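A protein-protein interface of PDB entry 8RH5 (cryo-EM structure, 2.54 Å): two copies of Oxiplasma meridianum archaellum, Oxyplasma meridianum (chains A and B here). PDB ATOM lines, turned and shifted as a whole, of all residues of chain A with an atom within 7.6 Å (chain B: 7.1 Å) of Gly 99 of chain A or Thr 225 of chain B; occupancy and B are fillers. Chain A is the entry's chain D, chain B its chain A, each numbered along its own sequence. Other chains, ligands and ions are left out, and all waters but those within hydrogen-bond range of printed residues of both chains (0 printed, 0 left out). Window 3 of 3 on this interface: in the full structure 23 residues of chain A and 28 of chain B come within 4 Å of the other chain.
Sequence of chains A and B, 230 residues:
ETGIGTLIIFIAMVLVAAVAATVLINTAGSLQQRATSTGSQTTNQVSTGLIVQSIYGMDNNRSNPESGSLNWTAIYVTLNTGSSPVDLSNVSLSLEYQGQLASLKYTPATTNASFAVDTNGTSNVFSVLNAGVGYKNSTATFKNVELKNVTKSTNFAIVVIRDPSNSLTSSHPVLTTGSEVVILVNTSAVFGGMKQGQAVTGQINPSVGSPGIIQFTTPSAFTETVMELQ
Among the printed residues, merely in contact across the chains: Glu 96 of chain A with Glu 224 of chain B (3.8 Å), Glu 96 of chain A with Val 226 of chain B (3.5 Å), Gly 99 of chain A with Thr 225 of chain B (3.8 Å), Gly 99 of chain A with Val 226 of chain B (3.7 Å) and Gln 100 of chain A with Asn 124 of chain B (3.7 Å).
No position is printed for both chains. Of the 6 pairs that touch across the chains among the printed residues, none has its exchanged pair printed and touching as well.
Thr 225 of chain B touches just one residue of chain A: Gly 99. Printed residues of chain B within 4 Å of Leu 101 of chain A: Asn 124 (3.3 Å). Of the printed residues of chain A, Val 226 of chain B touches Glu 96 (3.5 Å) and Gly 99 (3.7 Å). Of the printed residues of chain B, Glu 96 of chain A touches Glu 224 (3.8 Å) and Val 226 (3.5 Å). Ala 199 of chain A touches none of the printed residues of chain B. The nearest residue of chain B that does not touch Gly 99 of chain A is Arg 62 of chain B (4.2 Å).
N of Leu 101 of chain A sits at hydrogen-bond distance from OD1 of Asn 124 of chain B (3.3 Å).
O of Thr 225 of chain B lies within hydrogen-bond range of N of Asp 59 of chain B, at 2.8 Å. OE2 of Glu 96 of chain A lies within hydrogen-bond range of N of Gly 99 of chain A (3.4 Å).
Along chain A the printed residues that touch a printed residue of chain B span positions 96 to 101. Printed residues of chain B that touch a printed residue of chain A: Asn 124, Glu 224, Thr 225 and Val 226.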
ATOM      1  N   GLU A  96      -3.694 -14.476  37.493  1.00  0.00           N
ATOM      2  CA  GLU A  96      -3.138 -14.193  36.178  1.00  0.00           C
ATOM      3  C   GLU A  96      -3.565 -12.793  35.743  1.00  0.00           C
ATOM      4  O   GLU A  96      -4.758 -12.493  35.692  1.00  0.00           O
ATOM      5  CB  GLU A  96      -3.572 -15.269  35.177  1.00  0.00           C
ATOM      6  CG  GLU A  96      -2.637 -15.419  33.986  1.00  0.00           C
ATOM      7  CD  GLU A  96      -2.844 -14.443  32.840  1.00  0.00           C
ATOM      8  OE1 GLU A  96      -3.971 -14.383  32.305  1.00  0.00           O
ATOM      9  OE2 GLU A  96      -1.875 -13.745  32.481  1.00  0.00           O
ATOM     10  N   TYR A  97      -2.569 -11.951  35.434  1.00  0.00           N
ATOM     11  CA  TYR A  97      -2.783 -10.570  35.027  1.00  0.00           C
ATOM     12  C   TYR A  97      -1.629 -10.104  34.140  1.00  0.00           C
ATOM     13  O   TYR A  97      -0.480 -10.073  34.583  1.00  0.00           O
ATOM     14  CB  TYR A  97      -2.973  -9.669  36.253  1.00  0.00           C
ATOM     15  CG  TYR A  97      -3.022  -8.187  35.973  1.00  0.00           C
ATOM     16  CD1 TYR A  97      -4.200  -7.569  35.574  1.00  0.00           C
ATOM     17  CD2 TYR A  97      -1.892  -7.393  36.118  1.00  0.00           C
ATOM     18  CE1 TYR A  97      -4.252  -6.207  35.317  1.00  0.00           C
ATOM     19  CE2 TYR A  97      -1.926  -6.029  35.862  1.00  0.00           C
ATOM     20  CZ  TYR A  97      -3.111  -5.435  35.462  1.00  0.00           C
ATOM     21  OH  TYR A  97      -3.152  -4.094  35.209  1.00  0.00           O
ATOM     22  N   GLN A  98      -1.969  -9.743  32.892  1.00  0.00           N
ATOM     23  CA  GLN A  98      -1.092  -9.101  31.919  1.00  0.00           C
ATOM     24  C   GLN A  98       0.225  -9.863  31.763  1.00  0.00           C
ATOM     25  O   GLN A  98       1.302  -9.273  31.833  1.00  0.00           O
ATOM     26  CB  GLN A  98      -0.885  -7.620  32.255  1.00  0.00           C
ATOM     27  CG  GLN A  98      -2.057  -6.728  31.870  1.00  0.00           C
ATOM     28  CD  GLN A  98      -1.713  -5.257  31.872  1.00  0.00           C
ATOM     29  OE1 GLN A  98      -0.973  -4.766  32.723  1.00  0.00           O
ATOM     30  NE2 GLN A  98      -2.265  -4.532  30.913  1.00  0.00           N
ATOM     31  N   GLY A  99       0.116 -11.180  31.544  1.00  0.00           N
ATOM     32  CA  GLY A  99       1.263 -12.041  31.302  1.00  0.00           C
ATOM     33  C   GLY A  99       2.136 -12.229  32.540  1.00  0.00           C
ATOM     34  O   GLY A  99       3.363 -12.240  32.437  1.00  0.00           O
ATOM     35  N   GLN A 100       1.483 -12.370  33.701  1.00  0.00           N
ATOM     36  CA  GLN A 100       2.148 -12.615  34.971  1.00  0.00           C
ATOM     37  C   GLN A 100       1.283 -13.563  35.797  1.00  0.00           C
ATOM     38  O   GLN A 100       0.155 -13.227  36.155  1.00  0.00           O
ATOM     39  CB  GLN A 100       2.418 -11.291  35.695  1.00  0.00           C
ATOM     40  CG  GLN A 100       3.450 -11.391  36.809  1.00  0.00           C
ATOM     41  CD  GLN A 100       3.601 -10.109  37.592  1.00  0.00           C
ATOM     42  OE1 GLN A 100       3.797  -9.030  37.034  1.00  0.00           O
ATOM     43  NE2 GLN A 100       3.525 -10.220  38.909  1.00  0.00           N
ATOM     44  N   LEU A 101       1.829 -14.755  36.072  1.00  0.00           N
ATOM     45  CA  LEU A 101       1.138 -15.791  36.823  1.00  0.00           C
ATOM     46  C   LEU A 101       1.723 -15.861  38.232  1.00  0.00           C
ATOM     47  O   LEU A 101       2.862 -16.285  38.416  1.00  0.00           O
ATOM     48  CB  LEU A 101       1.277 -17.124  36.074  1.00  0.00           C
ATOM     49  CG  LEU A 101       0.427 -18.286  36.589  1.00  0.00           C
ATOM     50  CD1 LEU A 101      -1.017 -18.167  36.125  1.00  0.00           C
ATOM     51  CD2 LEU A 101       1.012 -19.617  36.141  1.00  0.00           C
ATOM     52  N   ALA A 102       0.920 -15.432  39.215  1.00  0.00           N
ATOM     53  CA  ALA A 102       1.337 -15.340  40.606  1.00  0.00           C
ATOM     54  C   ALA A 102       0.883 -16.575  41.380  1.00  0.00           C
ATOM     55  O   ALA A 102      -0.128 -17.189  41.041  1.00  0.00           O
ATOM     56  CB  ALA A 102       0.789 -14.074  41.218  1.00  0.00           C
ATOM     57  N   PHE A 191       1.434  -6.930  41.249  1.00  0.00           N
ATOM     58  CA  PHE A 191       1.302  -6.567  39.846  1.00  0.00           C
ATOM     59  C   PHE A 191       1.758  -5.128  39.605  1.00  0.00           C
ATOM     60  O   PHE A 191       2.088  -4.768  38.475  1.00  0.00           O
ATOM     61  CB  PHE A 191      -0.130  -6.801  39.353  1.00  0.00           C
ATOM     62  CG  PHE A 191      -0.641  -8.214  39.503  1.00  0.00           C
ATOM     63  CD1 PHE A 191      -0.088  -9.256  38.770  1.00  0.00           C
ATOM     64  CD2 PHE A 191      -1.688  -8.500  40.370  1.00  0.00           C
ATOM     65  CE1 PHE A 191      -0.562 -10.554  38.910  1.00  0.00           C
ATOM     66  CE2 PHE A 191      -2.163  -9.798  40.508  1.00  0.00           C
ATOM     67  CZ  PHE A 191      -1.600 -10.823  39.776  1.00  0.00           C
ATOM     68  N   ALA A 199      -8.486  -8.112  32.220  1.00  0.00           N
ATOM     69  CA  ALA A 199      -9.060  -9.377  32.654  1.00  0.00           C
ATOM     70  C   ALA A 199      -8.191 -10.006  33.743  1.00  0.00           C
ATOM     71  O   ALA A 199      -6.967 -10.045  33.621  1.00  0.00           O
ATOM     72  CB  ALA A 199      -9.229 -10.300  31.473  1.00  0.00           C
ATOM     73  N   GLY B  57       0.471 -21.655  29.137  1.00  0.00           N
ATOM     74  CA  GLY B  57       1.458 -21.383  28.104  1.00  0.00           C
ATOM     75  C   GLY B  57       1.841 -19.906  28.050  1.00  0.00           C
ATOM     76  O   GLY B  57       1.077 -19.047  28.492  1.00  0.00           O
ATOM     77  N   MET B  58       3.029 -19.629  27.494  1.00  0.00           N
ATOM     78  CA  MET B  58       3.573 -18.282  27.404  1.00  0.00           C
ATOM     79  C   MET B  58       3.986 -17.992  25.961  1.00  0.00           C
ATOM     80  O   MET B  58       4.713 -18.775  25.353  1.00  0.00           O
ATOM     81  CB  MET B  58       4.781 -18.123  28.338  1.00  0.00           C
ATOM     82  CG  MET B  58       5.267 -16.688  28.481  1.00  0.00           C
ATOM     83  SD  MET B  58       6.361 -16.433  29.909  1.00  0.00           S
ATOM     84  CE  MET B  58       7.875 -17.192  29.325  1.00  0.00           C
ATOM     85  N   ASP B  59       3.512 -16.851  25.441  1.00  0.00           N
ATOM     86  CA  ASP B  59       3.810 -16.387  24.093  1.00  0.00           C
ATOM     87  C   ASP B  59       5.205 -15.765  24.067  1.00  0.00           C
ATOM     88  O   ASP B  59       5.661 -15.228  25.076  1.00  0.00           O
ATOM     89  CB  ASP B  59       2.740 -15.405  23.604  1.00  0.00           C
ATOM     90  CG  ASP B  59       2.723 -15.219  22.096  1.00  0.00           C
ATOM     91  OD1 ASP B  59       2.215 -16.120  21.400  1.00  0.00           O
ATOM     92  OD2 ASP B  59       3.223 -14.176  21.632  1.00  0.00           O
ATOM     93  N   ASN B  60       5.860 -15.830  22.899  1.00  0.00           N
ATOM     94  CA  ASN B  60       7.249 -15.419  22.747  1.00  0.00           C
ATOM     95  C   ASN B  60       7.351 -13.950  22.326  1.00  0.00           C
ATOM     96  O   ASN B  60       8.432 -13.367  22.393  1.00  0.00           O
ATOM     97  CB  ASN B  60       8.042 -16.371  21.843  1.00  0.00           C
ATOM     98  CG  ASN B  60       7.743 -16.228  20.364  1.00  0.00           C
ATOM     99  OD1 ASN B  60       6.602 -15.995  19.966  1.00  0.00           O
ATOM    100  ND2 ASN B  60       8.765 -16.377  19.536  1.00  0.00           N
ATOM    101  N   ASN B  61       6.224 -13.369  21.895  1.00  0.00           N
ATOM    102  CA  ASN B  61       6.167 -11.976  21.478  1.00  0.00           C
ATOM    103  C   ASN B  61       5.335 -11.185  22.485  1.00  0.00           C
ATOM    104  O   ASN B  61       4.193 -11.543  22.769  1.00  0.00           O
ATOM    105  CB  ASN B  61       5.658 -11.838  20.038  1.00  0.00           C
ATOM    106  CG  ASN B  61       5.989 -10.509  19.387  1.00  0.00           C
ATOM    107  OD1 ASN B  61       5.717  -9.447  19.948  1.00  0.00           O
ATOM    108  ND2 ASN B  61       6.566 -10.564  18.195  1.00  0.00           N
ATOM    109  N   ARG B  62       5.934 -10.108  23.009  1.00  0.00           N
ATOM    110  CA  ARG B  62       5.321  -9.259  24.020  1.00  0.00           C
ATOM    111  C   ARG B  62       4.664  -8.048  23.358  1.00  0.00           C
ATOM    112  O   ARG B  62       3.587  -7.627  23.775  1.00  0.00           O
ATOM    113  CB  ARG B  62       6.357  -8.855  25.075  1.00  0.00           C
ATOM    114  CG  ARG B  62       5.784  -8.111  26.275  1.00  0.00           C
ATOM    115  CD  ARG B  62       6.779  -7.943  27.409  1.00  0.00           C
ATOM    116  NE  ARG B  62       6.863  -9.125  28.262  1.00  0.00           N
ATOM    117  CZ  ARG B  62       6.123  -9.347  29.346  1.00  0.00           C
ATOM    118  NH1 ARG B  62       6.292 -10.459  30.039  1.00  0.00           N
ATOM    119  NH2 ARG B  62       5.217  -8.467  29.737  1.00  0.00           N
ATOM    120  N   SER B  63       5.329  -7.507  22.327  1.00  0.00           N
ATOM    121  CA  SER B  63       4.893  -6.308  21.622  1.00  0.00           C
ATOM    122  C   SER B  63       3.600  -6.569  20.853  1.00  0.00           C
ATOM    123  O   SER B  63       2.681  -5.753  20.894  1.00  0.00           O
ATOM    124  CB  SER B  63       5.982  -5.778  20.722  1.00  0.00           C
ATOM    125  OG  SER B  63       7.125  -5.401  21.476  1.00  0.00           O
ATOM    126  N   PRO B  65       1.341 -10.123  20.490  1.00  0.00           N
ATOM    127  CA  PRO B  65       1.181 -11.559  20.749  1.00  0.00           C
ATOM    128  C   PRO B  65       0.409 -12.325  19.675  1.00  0.00           C
ATOM    129  O   PRO B  65       0.289 -13.549  19.756  1.00  0.00           O
ATOM    130  CB  PRO B  65       0.410 -11.590  22.078  1.00  0.00           C
ATOM    131  CG  PRO B  65      -0.396 -10.309  22.075  1.00  0.00           C
ATOM    132  CD  PRO B  65       0.471  -9.301  21.349  1.00  0.00           C
ATOM    133  N   LEU B  70       4.215 -20.207  21.293  1.00  0.00           N
ATOM    134  CA  LEU B  70       4.450 -20.624  22.668  1.00  0.00           C
ATOM    135  C   LEU B  70       5.886 -21.123  22.815  1.00  0.00           C
ATOM    136  O   LEU B  70       6.308 -22.021  22.087  1.00  0.00           O
ATOM    137  CB  LEU B  70       3.434 -21.705  23.058  1.00  0.00           C
ATOM    138  CG  LEU B  70       1.966 -21.273  23.101  1.00  0.00           C
ATOM    139  CD1 LEU B  70       1.044 -22.477  22.985  1.00  0.00           C
ATOM    140  CD2 LEU B  70       1.653 -20.485  24.366  1.00  0.00           C
ATOM    141  N   ASN B  71       6.621 -20.529  23.765  1.00  0.00           N
ATOM    142  CA  ASN B  71       8.020 -20.861  23.994  1.00  0.00           C
ATOM    143  C   ASN B  71       8.190 -21.682  25.274  1.00  0.00           C
ATOM    144  O   ASN B  71       9.162 -22.426  25.397  1.00  0.00           O
ATOM    145  CB  ASN B  71       8.945 -19.638  23.892  1.00  0.00           C
ATOM    146  CG  ASN B  71       8.725 -18.565  24.942  1.00  0.00           C
ATOM    147  OD1 ASN B  71       7.679 -18.513  25.590  1.00  0.00           O
ATOM    148  ND2 ASN B  71       9.718 -17.700  25.105  1.00  0.00           N
ATOM    149  N   ASN B 124       5.673 -14.137  40.170  1.00  0.00           N
ATOM    150  CA  ASN B 124       5.681 -14.683  38.821  1.00  0.00           C
ATOM    151  C   ASN B 124       6.293 -16.081  38.843  1.00  0.00           C
ATOM    152  O   ASN B 124       7.378 -16.280  39.392  1.00  0.00           O
ATOM    153  CB  ASN B 124       6.380 -13.750  37.825  1.00  0.00           C
ATOM    154  CG  ASN B 124       6.156 -14.129  36.375  1.00  0.00           C
ATOM    155  OD1 ASN B 124       5.079 -14.584  35.996  1.00  0.00           O
ATOM    156  ND2 ASN B 124       7.170 -13.931  35.548  1.00  0.00           N
ATOM    157  N   PHE B 126       6.949 -17.783  35.992  1.00  0.00           N
ATOM    158  CA  PHE B 126       7.850 -17.835  34.850  1.00  0.00           C
ATOM    159  C   PHE B 126       9.114 -17.007  35.098  1.00  0.00           C
ATOM    160  O   PHE B 126       9.840 -16.692  34.157  1.00  0.00           O
ATOM    161  CB  PHE B 126       7.122 -17.393  33.575  1.00  0.00           C
ATOM    162  CG  PHE B 126       6.111 -18.373  33.036  1.00  0.00           C
ATOM    163  CD1 PHE B 126       6.509 -19.454  32.259  1.00  0.00           C
ATOM    164  CD2 PHE B 126       4.755 -18.208  33.289  1.00  0.00           C
ATOM    165  CE1 PHE B 126       5.577 -20.355  31.761  1.00  0.00           C
ATOM    166  CE2 PHE B 126       3.822 -19.105  32.789  1.00  0.00           C
ATOM    167  CZ  PHE B 126       4.235 -20.177  32.025  1.00  0.00           C
ATOM    168  N   PHE B 222      -3.841 -16.084  19.536  1.00  0.00           N
ATOM    169  CA  PHE B 222      -3.190 -15.694  20.777  1.00  0.00           C
ATOM    170  C   PHE B 222      -3.341 -14.185  20.956  1.00  0.00           C
ATOM    171  O   PHE B 222      -2.871 -13.408  20.124  1.00  0.00           O
ATOM    172  CB  PHE B 222      -1.721 -16.133  20.800  1.00  0.00           C
ATOM    173  CG  PHE B 222      -1.440 -17.580  20.469  1.00  0.00           C
ATOM    174  CD1 PHE B 222      -2.191 -18.612  21.020  1.00  0.00           C
ATOM    175  CD2 PHE B 222      -0.386 -17.916  19.627  1.00  0.00           C
ATOM    176  CE1 PHE B 222      -1.914 -19.938  20.717  1.00  0.00           C
ATOM    177  CE2 PHE B 222      -0.106 -19.242  19.327  1.00  0.00           C
ATOM    178  CZ  PHE B 222      -0.873 -20.251  19.870  1.00  0.00           C
ATOM    179  N   THR B 223      -4.006 -13.789  22.049  1.00  0.00           N
ATOM    180  CA  THR B 223      -4.384 -12.402  22.287  1.00  0.00           C
ATOM    181  C   THR B 223      -3.636 -11.833  23.492  1.00  0.00           C
ATOM    182  O   THR B 223      -3.430 -10.622  23.570  1.00  0.00           O
ATOM    183  CB  THR B 223      -5.907 -12.244  22.409  1.00  0.00           C
ATOM    184  OG1 THR B 223      -6.397 -13.182  23.369  1.00  0.00           O
ATOM    185  CG2 THR B 223      -6.634 -12.425  21.093  1.00  0.00           C
ATOM    186  N   GLU B 224      -3.243 -12.713  24.420  1.00  0.00           N
ATOM    187  CA  GLU B 224      -2.523 -12.323  25.626  1.00  0.00           C
ATOM    188  C   GLU B 224      -1.231 -13.130  25.752  1.00  0.00           C
ATOM    189  O   GLU B 224      -1.043 -14.124  25.049  1.00  0.00           O
ATOM    190  CB  GLU B 224      -3.431 -12.401  26.860  1.00  0.00           C
ATOM    191  CG  GLU B 224      -4.050 -13.770  27.100  1.00  0.00           C
ATOM    192  CD  GLU B 224      -5.180 -13.839  28.115  1.00  0.00           C
ATOM    193  OE1 GLU B 224      -5.242 -12.964  29.006  1.00  0.00           O
ATOM    194  OE2 GLU B 224      -6.000 -14.772  28.014  1.00  0.00           O
ATOM    195  N   THR B 225      -0.353 -12.682  26.663  1.00  0.00           N
ATOM    196  CA  THR B 225       0.988 -13.225  26.839  1.00  0.00           C
ATOM    197  C   THR B 225       0.919 -14.607  27.491  1.00  0.00           C
ATOM    198  O   THR B 225       1.498 -15.559  26.970  1.00  0.00           O
ATOM    199  CB  THR B 225       1.896 -12.224  27.570  1.00  0.00           C
ATOM    200  OG1 THR B 225       1.821 -10.966  26.899  1.00  0.00           O
ATOM    201  CG2 THR B 225       3.341 -12.665  27.645  1.00  0.00           C
ATOM    202  N   VAL B 226       0.218 -14.697  28.630  1.00  0.00           N
ATOM    203  CA  VAL B 226       0.026 -15.953  29.340  1.00  0.00           C
ATOM    204  C   VAL B 226      -1.429 -16.392  29.173  1.00  0.00           C
ATOM    205  O   VAL B 226      -2.350 -15.625  29.447  1.00  0.00           O
ATOM    206  CB  VAL B 226       0.462 -15.855  30.820  1.00  0.00           C
ATOM    207  CG1 VAL B 226      -0.017 -17.033  31.657  1.00  0.00           C
ATOM    208  CG2 VAL B 226       1.970 -15.700  30.954  1.00  0.00           C
ATOM    209  N   MET B 227      -1.603 -17.640  28.714  1.00  0.00           N
ATOM    210  CA  MET B 227      -2.904 -18.204  28.387  1.00  0.00           C
ATOM    211  C   MET B 227      -3.095 -19.530  29.119  1.00  0.00           C
ATOM    212  O   MET B 227      -2.131 -20.255  29.363  1.00  0.00           O
ATOM    213  CB  MET B 227      -3.027 -18.451  26.880  1.00  0.00           C
ATOM    214  CG  MET B 227      -3.127 -17.181  26.057  1.00  0.00           C
ATOM    215  SD  MET B 227      -2.738 -17.432  24.307  1.00  0.00           S
ATOM    216  CE  MET B 227      -0.947 -17.502  24.365  1.00  0.00           C
